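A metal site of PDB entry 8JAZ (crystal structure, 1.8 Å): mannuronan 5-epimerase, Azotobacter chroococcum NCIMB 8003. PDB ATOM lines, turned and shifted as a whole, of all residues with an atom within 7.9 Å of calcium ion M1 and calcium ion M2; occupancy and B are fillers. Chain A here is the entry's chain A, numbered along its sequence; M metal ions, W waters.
Water W2 lies within hydrogen-bond range of the side-chain carboxylate (OD2) of Asp 402 (2.7 Å), the backbone carbonyl oxygen (O) of Asp 396 (2.9 Å) and the backbone NH (N) of Gly 366 (3.5 Å).
The side-chain carboxylate of Asp 402 is in hydrogen-bond range of the backbone NH of Thr 398 (2.8 Å).
The backbone carbonyl oxygen of Asp 370 sits at hydrogen-bond distance from the backbone NH of Leu 403 (2.9 Å).
The backbone NH (N) of Gly 366 lies within hydrogen-bond range of the side-chain carboxylate (OD2) of Asp 396, at 2.7 Å.
The backbone carbonyl oxygen (O) of Asp 352 lies within hydrogen-bond range of the backbone NH (N) of Thr 371, at 2.9 Å.
N of Ala 334 is in hydrogen-bond range of OD1 of Asp 352.
The side-chain carboxylate (OD1) of Asp 396 sits at hydrogen-bond distance from the backbone NH (N) of Gly 365, 2.8 Å away.
The nearest printed residue that does not touch calcium ion M2 is Ala 349 (4.2 Å).
Calcium ion M2 is bound by O of Ala 348, at 2.2 Å.
OD2 of Asp 370 is bound to calcium ion M2 (2.2 Å).
The backbone carbonyl oxygen (O) of Gly 367 is bound to calcium ion M2.
The backbone carbonyl oxygen (O) of Gly 365 is bound to calcium ion M2.
O of Gly 350 is bound to calcium ion M2 (2.5 Å).
OD2 of Asp 352 binds calcium ion M2 (2.5 Å).
OD1 of Asp 370 is bound to calcium ion M2 (2.9 Å).
Calcium ion M2 has seven donor atoms within binding distance.
Five residues have an atom within 4 Å of calcium ion M1: Gly 366, Gly 367, Gly 368, Asp 370 and Asp 402.
Calcium ion M1 is bound by water W1, OD1 of Asp 370, O of Gly 368, OD1 of Asp 402, O of Gly 366 and water W2.
Calcium ion M1 has six donor atoms within binding distance.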
ATOM      1  N   VAL A 330      -9.397 -12.675  14.126  1.00  0.00           N
ATOM      2  CA  VAL A 330      -9.577 -13.822  13.245  1.00  0.00           C
ATOM      3  C   VAL A 330     -10.940 -14.408  13.552  1.00  0.00           C
ATOM      4  O   VAL A 330     -11.180 -14.912  14.651  1.00  0.00           O
ATOM      5  CB  VAL A 330      -8.470 -14.870  13.432  1.00  0.00           C
ATOM      6  CG1 VAL A 330      -8.465 -15.850  12.269  1.00  0.00           C
ATOM      7  CG2 VAL A 330      -7.117 -14.191  13.587  1.00  0.00           C
ATOM      8  N   GLY A 332     -12.436 -17.154  12.838  1.00  0.00           N
ATOM      9  CA  GLY A 332     -12.424 -18.558  12.483  1.00  0.00           C
ATOM     10  C   GLY A 332     -11.222 -19.257  13.095  1.00  0.00           C
ATOM     11  O   GLY A 332     -10.470 -18.677  13.889  1.00  0.00           O
ATOM     12  N   ALA A 333     -11.057 -20.522  12.708  1.00  0.00           N
ATOM     13  CA  ALA A 333     -10.008 -21.353  13.284  1.00  0.00           C
ATOM     14  C   ALA A 333      -8.638 -20.923  12.761  1.00  0.00           C
ATOM     15  O   ALA A 333      -8.461 -20.670  11.565  1.00  0.00           O
ATOM     16  CB  ALA A 333     -10.259 -22.823  12.963  1.00  0.00           C
ATOM     17  N   ALA A 334      -7.672 -20.851  13.676  1.00  0.00           N
ATOM     18  CA  ALA A 334      -6.284 -20.557  13.333  1.00  0.00           C
ATOM     19  C   ALA A 334      -5.413 -21.748  13.725  1.00  0.00           C
ATOM     20  O   ALA A 334      -5.440 -22.188  14.887  1.00  0.00           O
ATOM     21  CB  ALA A 334      -5.802 -19.286  14.041  1.00  0.00           C
ATOM     22  N   ASP A 346      -0.793 -16.310  19.468  1.00  0.00           N
ATOM     23  CA  ASP A 346      -2.047 -15.855  20.042  1.00  0.00           C
ATOM     24  C   ASP A 346      -3.189 -16.211  19.098  1.00  0.00           C
ATOM     25  O   ASP A 346      -3.168 -15.831  17.922  1.00  0.00           O
ATOM     26  CB  ASP A 346      -2.027 -14.345  20.302  1.00  0.00           C
ATOM     27  CG  ASP A 346      -1.046 -13.955  21.395  1.00  0.00           C
ATOM     28  OD1 ASP A 346      -0.520 -14.864  22.065  1.00  0.00           O
ATOM     29  OD2 ASP A 346      -0.810 -12.741  21.576  1.00  0.00           O
ATOM     30  N   GLY A 347      -4.182 -16.923  19.624  1.00  0.00           N
ATOM     31  CA  GLY A 347      -5.390 -17.211  18.879  1.00  0.00           C
ATOM     32  C   GLY A 347      -6.378 -16.065  18.928  1.00  0.00           C
ATOM     33  O   GLY A 347      -6.109 -14.980  19.439  1.00  0.00           O
ATOM     34  N   ALA A 348      -7.561 -16.330  18.381  1.00  0.00           N
ATOM     35  CA  ALA A 348      -8.617 -15.329  18.280  1.00  0.00           C
ATOM     36  C   ALA A 348      -9.956 -16.015  18.552  1.00  0.00           C
ATOM     37  O   ALA A 348     -10.004 -17.107  19.134  1.00  0.00           O
ATOM     38  CB  ALA A 348      -8.574 -14.618  16.922  1.00  0.00           C
ATOM     39  N   ALA A 349     -11.045 -15.371  18.150  1.00  0.00           N
ATOM     40  CA  ALA A 349     -12.388 -15.816  18.525  1.00  0.00           C
ATOM     41  C   ALA A 349     -12.717 -17.213  18.035  1.00  0.00           C
ATOM     42  O   ALA A 349     -13.652 -17.833  18.557  1.00  0.00           O
ATOM     43  CB  ALA A 349     -13.419 -14.824  17.994  1.00  0.00           C
ATOM     44  N   GLY A 350     -11.996 -17.741  17.045  1.00  0.00           N
ATOM     45  CA  GLY A 350     -12.270 -19.060  16.530  1.00  0.00           C
ATOM     46  C   GLY A 350     -11.731 -20.165  17.424  1.00  0.00           C
ATOM     47  O   GLY A 350     -11.098 -19.937  18.455  1.00  0.00           O
ATOM     48  N   ASN A 351     -12.005 -21.406  17.006  1.00  0.00           N
ATOM     49  CA  ASN A 351     -11.517 -22.594  17.708  1.00  0.00           C
ATOM     50  C   ASN A 351     -10.154 -22.941  17.149  1.00  0.00           C
ATOM     51  O   ASN A 351     -10.036 -23.554  16.092  1.00  0.00           O
ATOM     52  CB  ASN A 351     -12.499 -23.754  17.549  1.00  0.00           C
ATOM     53  CG  ASN A 351     -13.813 -23.524  18.269  1.00  0.00           C
ATOM     54  OD1 ASN A 351     -13.942 -22.579  19.057  1.00  0.00           O
ATOM     55  ND2 ASN A 351     -14.795 -24.378  18.004  1.00  0.00           N
ATOM     56  N   ASP A 352      -9.103 -22.568  17.874  1.00  0.00           N
ATOM     57  CA  ASP A 352      -7.745 -22.598  17.358  1.00  0.00           C
ATOM     58  C   ASP A 352      -6.964 -23.797  17.898  1.00  0.00           C
ATOM     59  O   ASP A 352      -7.289 -24.359  18.947  1.00  0.00           O
ATOM     60  CB  ASP A 352      -7.009 -21.305  17.704  1.00  0.00           C
ATOM     61  CG  ASP A 352      -7.757 -20.073  17.262  1.00  0.00           C
ATOM     62  OD1 ASP A 352      -8.259 -20.053  16.121  1.00  0.00           O
ATOM     63  OD2 ASP A 352      -7.853 -19.123  18.070  1.00  0.00           O
ATOM     64  N   LEU A 353      -5.934 -24.175  17.147  1.00  0.00           N
ATOM     65  CA  LEU A 353      -4.945 -25.157  17.571  1.00  0.00           C
ATOM     66  C   LEU A 353      -3.615 -24.443  17.744  1.00  0.00           C
ATOM     67  O   LEU A 353      -3.175 -23.720  16.850  1.00  0.00           O
ATOM     68  CB  LEU A 353      -4.821 -26.280  16.528  1.00  0.00           C
ATOM     69  CG  LEU A 353      -3.685 -27.284  16.723  1.00  0.00           C
ATOM     70  CD1 LEU A 353      -3.854 -28.057  18.022  1.00  0.00           C
ATOM     71  CD2 LEU A 353      -3.574 -28.217  15.523  1.00  0.00           C
ATOM     72  N   LEU A 354      -2.981 -24.642  18.901  1.00  0.00           N
ATOM     73  CA  LEU A 354      -1.705 -24.000  19.187  1.00  0.00           C
ATOM     74  C   LEU A 354      -0.688 -25.049  19.609  1.00  0.00           C
ATOM     75  O   LEU A 354      -0.964 -25.882  20.471  1.00  0.00           O
ATOM     76  CB  LEU A 354      -1.848 -22.944  20.280  1.00  0.00           C
ATOM     77  CG  LEU A 354      -2.792 -21.774  19.993  1.00  0.00           C
ATOM     78  CD1 LEU A 354      -4.167 -22.030  20.589  1.00  0.00           C
ATOM     79  CD2 LEU A 354      -2.205 -20.480  20.519  1.00  0.00           C
ATOM     80  N   SER A 364      -1.583 -18.294  23.720  1.00  0.00           N
ATOM     81  CA  SER A 364      -2.868 -17.814  24.197  1.00  0.00           C
ATOM     82  C   SER A 364      -3.927 -18.159  23.167  1.00  0.00           C
ATOM     83  O   SER A 364      -3.715 -17.997  21.956  1.00  0.00           O
ATOM     84  CB  SER A 364      -2.856 -16.299  24.459  1.00  0.00           C
ATOM     85  OG  SER A 364      -2.753 -15.566  23.244  1.00  0.00           O
ATOM     86  N   GLY A 365      -5.078 -18.626  23.642  1.00  0.00           N
ATOM     87  CA  GLY A 365      -6.117 -19.104  22.746  1.00  0.00           C
ATOM     88  C   GLY A 365      -7.148 -18.071  22.359  1.00  0.00           C
ATOM     89  O   GLY A 365      -7.774 -18.183  21.306  1.00  0.00           O
ATOM     90  N   GLY A 366      -7.340 -17.057  23.204  1.00  0.00           N
ATOM     91  CA  GLY A 366      -8.410 -16.106  22.927  1.00  0.00           C
ATOM     92  C   GLY A 366      -9.776 -16.734  23.135  1.00  0.00           C
ATOM     93  O   GLY A 366      -9.961 -17.664  23.927  1.00  0.00           O
ATOM     94  N   GLY A 367     -10.758 -16.217  22.408  1.00  0.00           N
ATOM     95  CA  GLY A 367     -12.099 -16.738  22.486  1.00  0.00           C
ATOM     96  C   GLY A 367     -12.224 -18.123  21.858  1.00  0.00           C
ATOM     97  O   GLY A 367     -11.338 -18.614  21.155  1.00  0.00           O
ATOM     98  N   GLY A 368     -13.363 -18.762  22.132  1.00  0.00           N
ATOM     99  CA  GLY A 368     -13.626 -20.075  21.598  1.00  0.00           C
ATOM    100  C   GLY A 368     -12.950 -21.176  22.398  1.00  0.00           C
ATOM    101  O   GLY A 368     -12.275 -20.952  23.409  1.00  0.00           O
ATOM    102  N   ALA A 369     -13.122 -22.403  21.909  1.00  0.00           N
ATOM    103  CA  ALA A 369     -12.524 -23.589  22.511  1.00  0.00           C
ATOM    104  C   ALA A 369     -11.237 -23.905  21.757  1.00  0.00           C
ATOM    105  O   ALA A 369     -11.269 -24.318  20.598  1.00  0.00           O
ATOM    106  CB  ALA A 369     -13.490 -24.772  22.483  1.00  0.00           C
ATOM    107  N   ASP A 370     -10.103 -23.727  22.432  1.00  0.00           N
ATOM    108  CA  ASP A 370      -8.792 -23.845  21.805  1.00  0.00           C
ATOM    109  C   ASP A 370      -8.054 -25.054  22.345  1.00  0.00           C
ATOM    110  O   ASP A 370      -8.117 -25.355  23.539  1.00  0.00           O
ATOM    111  CB  ASP A 370      -7.965 -22.581  22.053  1.00  0.00           C
ATOM    112  CG  ASP A 370      -8.676 -21.323  21.597  1.00  0.00           C
ATOM    113  OD1 ASP A 370      -9.070 -20.522  22.466  1.00  0.00           O
ATOM    114  OD2 ASP A 370      -8.842 -21.142  20.373  1.00  0.00           O
ATOM    115  N   THR A 371      -7.354 -25.749  21.460  1.00  0.00           N
ATOM    116  CA  THR A 371      -6.512 -26.881  21.825  1.00  0.00           C
ATOM    117  C   THR A 371      -5.060 -26.432  21.899  1.00  0.00           C
ATOM    118  O   THR A 371      -4.527 -25.876  20.928  1.00  0.00           O
ATOM    119  CB  THR A 371      -6.672 -28.030  20.827  1.00  0.00           C
ATOM    120  OG1 THR A 371      -8.009 -28.535  20.880  1.00  0.00           O
ATOM    121  CG2 THR A 371      -5.700 -29.154  21.160  1.00  0.00           C
ATOM    122  N   PHE A 372      -4.418 -26.672  23.044  1.00  0.00           N
ATOM    123  CA  PHE A 372      -2.996 -26.422  23.215  1.00  0.00           C
ATOM    124  C   PHE A 372      -2.303 -27.773  23.240  1.00  0.00           C
ATOM    125  O   PHE A 372      -2.405 -28.513  24.225  1.00  0.00           O
ATOM    126  CB  PHE A 372      -2.733 -25.636  24.501  1.00  0.00           C
ATOM    127  CG  PHE A 372      -3.475 -24.327  24.585  1.00  0.00           C
ATOM    128  CD1 PHE A 372      -2.880 -23.154  24.154  1.00  0.00           C
ATOM    129  CD2 PHE A 372      -4.756 -24.273  25.104  1.00  0.00           C
ATOM    130  CE1 PHE A 372      -3.553 -21.944  24.234  1.00  0.00           C
ATOM    131  CE2 PHE A 372      -5.436 -23.075  25.187  1.00  0.00           C
ATOM    132  CZ  PHE A 372      -4.838 -21.913  24.750  1.00  0.00           C
ATOM    133  N   ASP A 396      -4.222 -17.703  28.805  1.00  0.00           N
ATOM    134  CA  ASP A 396      -5.644 -17.494  29.077  1.00  0.00           C
ATOM    135  C   ASP A 396      -6.421 -18.803  29.012  1.00  0.00           C
ATOM    136  O   ASP A 396      -7.508 -18.871  28.437  1.00  0.00           O
ATOM    137  CB  ASP A 396      -6.236 -16.481  28.105  1.00  0.00           C
ATOM    138  CG  ASP A 396      -6.192 -16.956  26.669  1.00  0.00           C
ATOM    139  OD1 ASP A 396      -5.320 -17.802  26.349  1.00  0.00           O
ATOM    140  OD2 ASP A 396      -7.026 -16.497  25.858  1.00  0.00           O
ATOM    141  N   PHE A 397      -5.878 -19.867  29.611  1.00  0.00           N
ATOM    142  CA  PHE A 397      -6.582 -21.145  29.565  1.00  0.00           C
ATOM    143  C   PHE A 397      -7.886 -21.073  30.342  1.00  0.00           C
ATOM    144  O   PHE A 397      -7.931 -20.564  31.477  1.00  0.00           O
ATOM    145  CB  PHE A 397      -5.712 -22.271  30.130  1.00  0.00           C
ATOM    146  CG  PHE A 397      -6.249 -23.630  29.833  1.00  0.00           C
ATOM    147  CD1 PHE A 397      -7.084 -24.270  30.727  1.00  0.00           C
ATOM    148  CD2 PHE A 397      -5.937 -24.266  28.637  1.00  0.00           C
ATOM    149  CE1 PHE A 397      -7.598 -25.522  30.442  1.00  0.00           C
ATOM    150  CE2 PHE A 397      -6.438 -25.516  28.356  1.00  0.00           C
ATOM    151  CZ  PHE A 397      -7.267 -26.150  29.255  1.00  0.00           C
ATOM    152  N   THR A 398      -8.951 -21.588  29.741  1.00  0.00           N
ATOM    153  CA  THR A 398     -10.293 -21.580  30.328  1.00  0.00           C
ATOM    154  C   THR A 398     -10.735 -23.018  30.487  1.00  0.00           C
ATOM    155  O   THR A 398     -11.038 -23.686  29.482  1.00  0.00           O
ATOM    156  CB  THR A 398     -11.294 -20.797  29.468  1.00  0.00           C
ATOM    157  OG1 THR A 398     -11.772 -21.624  28.407  1.00  0.00           O
ATOM    158  CG2 THR A 398     -10.633 -19.555  28.877  1.00  0.00           C
ATOM    159  N   ALA A 401     -13.778 -24.461  28.484  1.00  0.00           N
ATOM    160  CA  ALA A 401     -13.738 -24.496  27.026  1.00  0.00           C
ATOM    161  C   ALA A 401     -12.452 -25.076  26.463  1.00  0.00           C
ATOM    162  O   ALA A 401     -12.495 -25.955  25.594  1.00  0.00           O
ATOM    163  CB  ALA A 401     -13.953 -23.082  26.462  1.00  0.00           C
ATOM    164  N   ASP A 402     -11.294 -24.610  26.930  1.00  0.00           N
ATOM    165  CA  ASP A 402     -10.031 -24.976  26.307  1.00  0.00           C
ATOM    166  C   ASP A 402      -9.598 -26.384  26.707  1.00  0.00           C
ATOM    167  O   ASP A 402     -10.102 -26.985  27.667  1.00  0.00           O
ATOM    168  CB  ASP A 402      -8.943 -23.977  26.680  1.00  0.00           C
ATOM    169  CG  ASP A 402      -9.286 -22.556  26.266  1.00  0.00           C
ATOM    170  OD1 ASP A 402     -10.017 -22.394  25.261  1.00  0.00           O
ATOM    171  OD2 ASP A 402      -8.820 -21.621  26.940  1.00  0.00           O
ATOM    172  N   LEU A 403      -8.635 -26.920  25.941  1.00  0.00           N
ATOM    173  CA  LEU A 403      -8.160 -28.285  26.102  1.00  0.00           C
ATOM    174  C   LEU A 403      -6.643 -28.306  25.974  1.00  0.00           C
ATOM    175  O   LEU A 403      -6.084 -27.647  25.096  1.00  0.00           O
ATOM    176  CB  LEU A 403      -8.823 -29.201  25.062  1.00  0.00           C
ATOM    177  CG  LEU A 403      -8.703 -30.728  25.028  1.00  0.00           C
ATOM    178  CD1 LEU A 403      -7.325 -31.214  24.598  1.00  0.00           C
ATOM    179  CD2 LEU A 403      -9.103 -31.331  26.372  1.00  0.00           C
HETATM  180 CA    CA M   1     -10.281 -20.092  24.448  1.00  0.00          CA
HETATM  181 CA    CA M   2      -9.439 -19.015  20.052  1.00  0.00          CA
HETATM  182  O   HOH W   1     -11.996 -19.658  25.983  1.00  0.00           O
HETATM  183  O   HOH W   2      -7.883 -19.422  25.659  1.00  0.00           O
